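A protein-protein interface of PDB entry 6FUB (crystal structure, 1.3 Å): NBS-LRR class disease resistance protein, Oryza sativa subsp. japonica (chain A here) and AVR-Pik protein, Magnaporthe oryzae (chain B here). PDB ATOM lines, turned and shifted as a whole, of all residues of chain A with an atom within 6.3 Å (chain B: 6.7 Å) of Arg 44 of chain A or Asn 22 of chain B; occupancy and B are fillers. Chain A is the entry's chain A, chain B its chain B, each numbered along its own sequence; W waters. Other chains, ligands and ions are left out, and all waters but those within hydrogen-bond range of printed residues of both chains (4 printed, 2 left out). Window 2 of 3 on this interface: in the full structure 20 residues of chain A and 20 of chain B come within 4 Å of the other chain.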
ATOM      1  N   ILE A  13     -12.884 -13.266  -4.727  1.00  0.00           N
ATOM      2  CA  ILE A  13     -11.939 -13.052  -5.830  1.00  0.00           C
ATOM      3  C   ILE A  13     -11.114 -14.289  -5.931  1.00  0.00           C
ATOM      4  O   ILE A  13     -10.187 -14.479  -5.171  1.00  0.00           O
ATOM      5  CB  ILE A  13     -11.043 -11.829  -5.704  1.00  0.00           C
ATOM      6  CG1 ILE A  13     -11.843 -10.579  -5.365  1.00  0.00           C
ATOM      7  CG2 ILE A  13     -10.305 -11.619  -7.034  1.00  0.00           C
ATOM      8  CD1 ILE A  13     -10.994  -9.351  -5.261  1.00  0.00           C
ATOM      9  N   MET A  15      -8.180 -16.378  -6.372  1.00  0.00           N
ATOM     10  CA  MET A  15      -6.812 -15.919  -6.294  1.00  0.00           C
ATOM     11  C   MET A  15      -5.883 -17.012  -6.786  1.00  0.00           C
ATOM     12  O   MET A  15      -5.969 -18.137  -6.324  1.00  0.00           O
ATOM     13  CB  MET A  15      -6.462 -15.663  -4.828  1.00  0.00           C
ATOM     14  CG  MET A  15      -7.293 -14.693  -4.016  1.00  0.00           C
ATOM     15  SD  MET A  15      -6.940 -12.971  -4.438  1.00  0.00           S
ATOM     16  CE  MET A  15      -8.106 -12.306  -3.287  1.00  0.00           C
ATOM     17  N   ARG A  21      -3.324 -11.840  -3.878  1.00  0.00           N
ATOM     18  CA  ARG A  21      -3.854 -11.312  -2.616  1.00  0.00           C
ATOM     19  C   ARG A  21      -3.204  -9.993  -2.235  1.00  0.00           C
ATOM     20  O   ARG A  21      -3.875  -9.059  -1.890  1.00  0.00           O
ATOM     21  CB  ARG A  21      -3.718 -12.304  -1.468  1.00  0.00           C
ATOM     22  CG  ARG A  21      -4.480 -13.589  -1.611  1.00  0.00           C
ATOM     23  CD  ARG A  21      -4.347 -14.423  -0.343  1.00  0.00           C
ATOM     24  NE  ARG A  21      -5.182 -15.588  -0.605  1.00  0.00           N
ATOM     25  CZ  ARG A  21      -4.785 -16.706  -1.172  1.00  0.00           C
ATOM     26  NH1 ARG A  21      -3.499 -16.935  -1.492  1.00  0.00           N
ATOM     27  NH2 ARG A  21      -5.681 -17.642  -1.387  1.00  0.00           N
ATOM     28  N   ILE A  39      -8.534 -10.035   4.016  1.00  0.00           N
ATOM     29  CA  ILE A  39      -8.818 -11.227   3.204  1.00  0.00           C
ATOM     30  C   ILE A  39      -8.884 -12.415   4.126  1.00  0.00           C
ATOM     31  O   ILE A  39      -7.931 -12.684   4.858  1.00  0.00           O
ATOM     32  CB  ILE A  39      -7.777 -11.414   2.103  1.00  0.00           C
ATOM     33  CG1 ILE A  39      -7.895 -10.228   1.124  1.00  0.00           C
ATOM     34  CG2 ILE A  39      -8.037 -12.716   1.328  1.00  0.00           C
ATOM     35  CD1 ILE A  39      -6.934 -10.232  -0.034  1.00  0.00           C
ATOM     36  N   ALA A  40      -9.976 -13.167   4.057  1.00  0.00           N
ATOM     37  CA  ALA A  40     -10.120 -14.436   4.818  1.00  0.00           C
ATOM     38  C   ALA A  40     -11.063 -15.377   4.096  1.00  0.00           C
ATOM     39  O   ALA A  40     -11.025 -15.357   2.879  1.00  0.00           O
ATOM     40  CB  ALA A  40     -10.437 -14.172   6.306  1.00  0.00           C
ATOM     41  N   GLY A  41     -11.877 -16.157   4.750  1.00  0.00           N
ATOM     42  CA  GLY A  41     -12.723 -17.128   4.102  1.00  0.00           C
ATOM     43  C   GLY A  41     -12.039 -18.489   3.936  1.00  0.00           C
ATOM     44  O   GLY A  41     -10.813 -18.631   4.062  1.00  0.00           O
ATOM     45  N   ASP A  42     -12.837 -19.479   3.575  1.00  0.00           N
ATOM     46  CA  ASP A  42     -12.363 -20.859   3.479  1.00  0.00           C
ATOM     47  C   ASP A  42     -11.259 -21.034   2.428  1.00  0.00           C
ATOM     48  O   ASP A  42     -10.392 -21.887   2.604  1.00  0.00           O
ATOM     49  CB  ASP A  42     -13.510 -21.799   3.118  1.00  0.00           C
ATOM     50  CG  ASP A  42     -14.512 -22.005   4.244  1.00  0.00           C
ATOM     51  OD1 ASP A  42     -14.291 -21.641   5.462  1.00  0.00           O
ATOM     52  OD2 ASP A  42     -15.519 -22.680   3.970  1.00  0.00           O
ATOM     53  N   LEU A  43     -11.291 -20.208   1.378  1.00  0.00           N
ATOM     54  CA  LEU A  43     -10.258 -20.227   0.348  1.00  0.00           C
ATOM     55  C   LEU A  43      -9.294 -19.047   0.406  1.00  0.00           C
ATOM     56  O   LEU A  43      -8.542 -18.804  -0.528  1.00  0.00           O
ATOM     57  CB  LEU A  43     -10.933 -20.229  -1.052  1.00  0.00           C
ATOM     58  CG  LEU A  43     -11.623 -21.515  -1.423  1.00  0.00           C
ATOM     59  CD1 LEU A  43     -12.425 -21.341  -2.648  1.00  0.00           C
ATOM     60  CD2 LEU A  43     -10.554 -22.625  -1.591  1.00  0.00           C
ATOM     61  N   ARG A  44      -9.345 -18.275   1.475  1.00  0.00           N
ATOM     62  CA  ARG A  44      -8.617 -17.036   1.538  1.00  0.00           C
ATOM     63  C   ARG A  44      -8.858 -16.161   0.326  1.00  0.00           C
ATOM     64  O   ARG A  44      -7.937 -15.579  -0.231  1.00  0.00           O
ATOM     65  CB  ARG A  44      -7.146 -17.295   1.857  1.00  0.00           C
ATOM     66  CG  ARG A  44      -6.999 -17.742   3.294  1.00  0.00           C
ATOM     67  CD  ARG A  44      -5.982 -18.820   3.493  1.00  0.00           C
ATOM     68  NE  ARG A  44      -5.874 -19.063   4.920  1.00  0.00           N
ATOM     69  CZ  ARG A  44      -6.630 -19.882   5.657  1.00  0.00           C
ATOM     70  NH1 ARG A  44      -7.618 -20.602   5.169  1.00  0.00           N
ATOM     71  NH2 ARG A  44      -6.381 -19.972   6.951  1.00  0.00           N
ATOM     72  N   ASP A  45     -10.125 -16.079  -0.077  1.00  0.00           N
ATOM     73  CA  ASP A  45     -10.490 -15.310  -1.250  1.00  0.00           C
ATOM     74  C   ASP A  45     -11.685 -14.431  -1.008  1.00  0.00           C
ATOM     75  O   ASP A  45     -12.245 -13.892  -1.919  1.00  0.00           O
ATOM     76  CB  ASP A  45     -10.576 -16.199  -2.497  1.00  0.00           C
ATOM     77  CG  ASP A  45     -11.789 -17.037  -2.582  1.00  0.00           C
ATOM     78  OD1 ASP A  45     -12.655 -16.995  -1.677  1.00  0.00           O
ATOM     79  OD2 ASP A  45     -11.909 -17.743  -3.633  1.00  0.00           O
ATOM     80  N   GLN A  46     -12.036 -14.252   0.270  1.00  0.00           N
ATOM     81  CA  GLN A  46     -13.147 -13.417   0.672  1.00  0.00           C
ATOM     82  C   GLN A  46     -12.516 -12.098   1.073  1.00  0.00           C
ATOM     83  O   GLN A  46     -11.757 -12.039   2.016  1.00  0.00           O
ATOM     84  CB  GLN A  46     -13.879 -14.149   1.800  1.00  0.00           C
ATOM     85  CG  GLN A  46     -15.217 -13.764   2.184  1.00  0.00           C
ATOM     86  CD  GLN A  46     -15.814 -14.480   3.334  1.00  0.00           C
ATOM     87  OE1 GLN A  46     -16.081 -13.830   4.334  1.00  0.00           O
ATOM     88  NE2 GLN A  46     -16.103 -15.792   3.217  1.00  0.00           N
ATOM     89  N   ARG B  19     -15.959 -26.834  10.968  1.00  0.00           N
ATOM     90  CA  ARG B  19     -14.883 -25.992  11.484  1.00  0.00           C
ATOM     91  C   ARG B  19     -15.281 -24.552  11.462  1.00  0.00           C
ATOM     92  O   ARG B  19     -16.158 -24.116  10.611  1.00  0.00           O
ATOM     93  CB  ARG B  19     -13.599 -26.160  10.701  1.00  0.00           C
ATOM     94  CG  ARG B  19     -13.697 -25.557   9.305  1.00  0.00           C
ATOM     95  CD  ARG B  19     -12.596 -26.077   8.441  1.00  0.00           C
ATOM     96  NE  ARG B  19     -12.622 -25.472   7.113  1.00  0.00           N
ATOM     97  CZ  ARG B  19     -13.370 -25.897   6.111  1.00  0.00           C
ATOM     98  NH1 ARG B  19     -14.225 -26.878   6.265  1.00  0.00           N
ATOM     99  NH2 ARG B  19     -13.242 -25.306   4.977  1.00  0.00           N
ATOM    100  N   ASP B  20     -14.807 -23.710  12.303  1.00  0.00           N
ATOM    101  CA  ASP B  20     -15.175 -22.329  12.325  1.00  0.00           C
ATOM    102  C   ASP B  20     -14.897 -21.693  10.947  1.00  0.00           C
ATOM    103  O   ASP B  20     -14.016 -22.116  10.199  1.00  0.00           O
ATOM    104  CB  ASP B  20     -14.389 -21.511  13.347  1.00  0.00           C
ATOM    105  CG  ASP B  20     -14.804 -21.701  14.790  1.00  0.00           C
ATOM    106  OD1 ASP B  20     -15.792 -22.382  15.076  1.00  0.00           O
ATOM    107  OD2 ASP B  20     -13.996 -21.107  15.614  1.00  0.00           O
ATOM    108  N   PRO B  21     -15.664 -20.641  10.607  1.00  0.00           N
ATOM    109  CA  PRO B  21     -15.205 -19.795   9.523  1.00  0.00           C
ATOM    110  C   PRO B  21     -13.818 -19.239   9.659  1.00  0.00           C
ATOM    111  O   PRO B  21     -13.342 -19.127  10.863  1.00  0.00           O
ATOM    112  CB  PRO B  21     -16.230 -18.629   9.528  1.00  0.00           C
ATOM    113  CG  PRO B  21     -17.450 -19.184  10.224  1.00  0.00           C
ATOM    114  CD  PRO B  21     -16.785 -20.040  11.321  1.00  0.00           C
ATOM    115  N   ASN B  22     -13.091 -18.990   8.638  1.00  0.00           N
ATOM    116  CA  ASN B  22     -11.840 -18.348   8.675  1.00  0.00           C
ATOM    117  C   ASN B  22     -12.162 -16.863   8.672  1.00  0.00           C
ATOM    118  O   ASN B  22     -12.334 -16.291   7.597  1.00  0.00           O
ATOM    119  CB  ASN B  22     -10.964 -18.748   7.506  1.00  0.00           C
ATOM    120  CG  ASN B  22      -9.668 -17.974   7.483  1.00  0.00           C
ATOM    121  OD1 ASN B  22      -9.202 -17.535   8.564  1.00  0.00           O
ATOM    122  ND2 ASN B  22      -9.109 -17.756   6.296  1.00  0.00           N
ATOM    123  N   PHE B  23     -12.327 -16.282   9.845  1.00  0.00           N
ATOM    124  CA  PHE B  23     -12.821 -14.923  10.033  1.00  0.00           C
ATOM    125  C   PHE B  23     -11.695 -13.983  10.429  1.00  0.00           C
ATOM    126  O   PHE B  23     -10.649 -14.383  10.965  1.00  0.00           O
ATOM    127  CB  PHE B  23     -13.930 -14.891  11.102  1.00  0.00           C
ATOM    128  CG  PHE B  23     -13.497 -15.359  12.458  1.00  0.00           C
ATOM    129  CD1 PHE B  23     -12.974 -14.439  13.361  1.00  0.00           C
ATOM    130  CD2 PHE B  23     -13.653 -16.658  12.873  1.00  0.00           C
ATOM    131  CE1 PHE B  23     -12.537 -14.812  14.601  1.00  0.00           C
ATOM    132  CE2 PHE B  23     -13.194 -17.060  14.131  1.00  0.00           C
ATOM    133  CZ  PHE B  23     -12.659 -16.135  14.985  1.00  0.00           C
ATOM    134  N   PHE B  24     -11.961 -12.703  10.319  1.00  0.00           N
ATOM    135  CA  PHE B  24     -11.058 -11.684  10.800  1.00  0.00           C
ATOM    136  C   PHE B  24     -11.918 -10.583  11.415  1.00  0.00           C
ATOM    137  O   PHE B  24     -12.719  -9.997  10.699  1.00  0.00           O
ATOM    138  CB  PHE B  24     -10.241 -11.158   9.640  1.00  0.00           C
ATOM    139  CG  PHE B  24      -9.186 -10.202  10.063  1.00  0.00           C
ATOM    140  CD1 PHE B  24      -9.454  -8.845  10.191  1.00  0.00           C
ATOM    141  CD2 PHE B  24      -7.951 -10.681  10.409  1.00  0.00           C
ATOM    142  CE1 PHE B  24      -8.462  -7.968  10.635  1.00  0.00           C
ATOM    143  CE2 PHE B  24      -6.952  -9.819  10.848  1.00  0.00           C
ATOM    144  CZ  PHE B  24      -7.219  -8.462  10.971  1.00  0.00           C
ATOM    145  N   ARG B  44     -20.397 -27.483   1.910  1.00  0.00           N
ATOM    146  CA  ARG B  44     -19.987 -26.181   2.252  1.00  0.00           C
ATOM    147  C   ARG B  44     -19.249 -25.459   1.121  1.00  0.00           C
ATOM    148  O   ARG B  44     -18.315 -25.966   0.561  1.00  0.00           O
ATOM    149  CB  ARG B  44     -19.047 -26.288   3.510  1.00  0.00           C
ATOM    150  CG  ARG B  44     -18.588 -24.964   4.030  1.00  0.00           C
ATOM    151  CD  ARG B  44     -17.904 -25.195   5.408  1.00  0.00           C
ATOM    152  NE  ARG B  44     -17.059 -24.081   5.849  1.00  0.00           N
ATOM    153  CZ  ARG B  44     -16.589 -23.989   7.139  1.00  0.00           C
ATOM    154  NH1 ARG B  44     -17.044 -24.884   7.968  1.00  0.00           N
ATOM    155  NH2 ARG B  44     -15.774 -22.997   7.405  1.00  0.00           N
ATOM    156  N   ASP B  46     -18.618 -21.660   1.504  1.00  0.00           N
ATOM    157  CA  ASP B  46     -17.822 -20.719   2.229  1.00  0.00           C
ATOM    158  C   ASP B  46     -18.574 -20.424   3.505  1.00  0.00           C
ATOM    159  O   ASP B  46     -19.633 -20.976   3.796  1.00  0.00           O
ATOM    160  CB  ASP B  46     -17.426 -19.444   1.426  1.00  0.00           C
ATOM    161  CG  ASP B  46     -16.093 -18.802   1.835  1.00  0.00           C
ATOM    162  OD1 ASP B  46     -15.576 -19.133   2.927  1.00  0.00           O
ATOM    163  OD2 ASP B  46     -15.624 -17.900   1.083  1.00  0.00           O
ATOM    164  N   ALA B  47     -17.884 -19.603   4.342  1.00  0.00           N
ATOM    165  CA  ALA B  47     -18.393 -19.249   5.693  1.00  0.00           C
ATOM    166  C   ALA B  47     -17.842 -17.920   6.092  1.00  0.00           C
ATOM    167  O   ALA B  47     -16.810 -17.481   5.597  1.00  0.00           O
ATOM    168  CB  ALA B  47     -18.027 -20.331   6.718  1.00  0.00           C
ATOM    169  N   GLY B  48     -18.525 -17.268   7.002  1.00  0.00           N
ATOM    170  CA  GLY B  48     -18.055 -15.971   7.471  1.00  0.00           C
ATOM    171  C   GLY B  48     -18.711 -15.506   8.748  1.00  0.00           C
ATOM    172  O   GLY B  48     -19.280 -16.323   9.435  1.00  0.00           O
ATOM    173  N   THR B  49     -18.686 -14.214   8.978  1.00  0.00           N
ATOM    174  CA  THR B  49     -19.327 -13.644  10.155  1.00  0.00           C
ATOM    175  C   THR B  49     -20.408 -12.616   9.713  1.00  0.00           C
ATOM    176  O   THR B  49     -20.284 -11.963   8.663  1.00  0.00           O
ATOM    177  CB  THR B  49     -18.363 -12.939  11.104  1.00  0.00           C
ATOM    178  OG1 THR B  49     -17.667 -11.910  10.391  1.00  0.00           O
ATOM    179  CG2 THR B  49     -17.360 -13.932  11.652  1.00  0.00           C
HETATM  180  O   HOH W   1     -17.718 -12.663   6.377  1.00  0.00           O
HETATM  181  O   HOH W   2     -12.870 -17.895   0.825  1.00  0.00           O
HETATM  182  O   HOH W   3     -15.505 -24.229   1.711  1.00  0.00           O
HETATM  183  O   HOH W   4     -12.225 -22.370   7.199  1.00  0.00           O
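Water W2 lies within hydrogen-bond range of the side-chain carboxylate (OD1) of Asp 45 of chain A (2.7 Å), the side-chain carboxylate (OD2) of Asp 46 of chain B (2.8 Å), the backbone NH (N) of Leu 43 of chain A (2.9 Å) and the backbone NH (N) of Asp 42 of chain A (3.2 Å). Water W3 lies within hydrogen-bond range of OD2 of Asp 42 of chain A (2.7 Å) and O of Arg 44 of chain B (3.5 Å). Water W4 bridges the side-chain carboxylate of Asp 42 of chain A (2.8 Å) and the guanidinium group of Arg 19 of chain B (3.1 Å). Water W1 bridges the side-chain amide oxygen (OE1) of Gln 46 of chain A (2.9 Å) and the backbone NH (N) of Thr 49 of chain B (3.2 Å).
The guanidinium group (NH1) of Arg 44 of chain B sits at hydrogen-bond distance from the backbone carbonyl oxygen (O) of Arg 19 of chain B, at 2.9 Å. The guanidinium group (NH2) of Arg 44 of chain B sits at hydrogen-bond distance from the backbone carbonyl oxygen (O) of Asp 20 of chain B. The backbone carbonyl oxygen (O) of Arg 44 of chain A lies within hydrogen-bond range of the guanidinium group (NE) of Arg 21 of chain A, at 2.8 Å. The backbone carbonyl oxygen (O) of Ala 40 of chain A lies within hydrogen-bond range of the backbone NH (N) of Asp 45 of chain A, at 3.2 Å. O of Gln 46 of chain A sits at hydrogen-bond distance from N of Ala 40 of chain A.
Among the printed residues, merely in contact across the chains: Ala 40 of chain A with Asn 22 of chain B (3.1 Å), Gly 41 of chain A with Asp 46 of chain B (3.7 Å) and Asp 42 of chain A with Ala 47 of chain B (3.9 Å).
The guanidinium group (NH2) of Arg 19 of chain B lies within salt-bridge range of the side-chain carboxylate (OD2) of Asp 42 of chain A, at 3.6 Å. The backbone carbonyl oxygen (O) of Asn 22 of chain B lies within hydrogen-bond range of the backbone NH (N) of Gly 41 of chain A (2.9 Å). The side-chain amide nitrogen (ND2) of Asn 22 of chain B lies close to the guanidinium group (NH1) of Arg 44 of chain A (3.4 Å). The guanidinium group of Arg 44 of chain B lies within salt-bridge range of the side-chain carboxylate of Asp 42 of chain A, at 2.8 Å. The side-chain carboxylate (OD1) of Asp 46 of chain B lies within hydrogen-bond range of the backbone NH (N) of Asp 42 of chain A, at 2.8 Å. The side-chain amide nitrogen (NE2) of Gln 46 of chain A lies within hydrogen-bond range of the side-chain carboxylate (OD2) of Asp 46 of chain B (3.0 Å). The backbone carbonyl oxygen (O) of Ala 47 of chain B lies within hydrogen-bond range of the side-chain amide nitrogen (NE2) of Gln 46 of chain A (3.0 Å).
Of the 11 printed residues of chain B, 5 touch a printed residue of chain A. Hydrophobic or aromatic side chains of chain A within 4 Å of the printed part of chain B: Ala 40. Among the printed residues, 10 pairs touch across the chains. Among the printed residues, Asp or Glu carboxylates within 4 Å of a Lys or Arg side-chain nitrogen of the other chain: Asp 42 of chain A with Arg 19 of chain B and Asp 42 of chain A with Arg 44 of chain B.
Leu 43 of chain A touches none of the printed residues of chain B. Of the printed residues of chain B, Arg 44 of chain A touches Asn 22 (3.3 Å). Pro 21 of chain B touches none of the printed residues of chain A. Of the printed residues of chain A, Asp 46 of chain B touches Gly 41 (3.7 Å), Asp 42 (2.8 Å) and Gln 46 (3.0 Å). Of the printed residues of chain A, Ala 47 of chain B touches Asp 42 (3.9 Å) and Gln 46 (3.0 Å). The nearest printed residue of chain A that does not touch Asn 22 of chain B is Asp 42 of chain A (4.3 Å). The nearest printed residue of chain B that does not touch Gln 46 of chain A is Gly 48 of chain B (4.3 Å).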
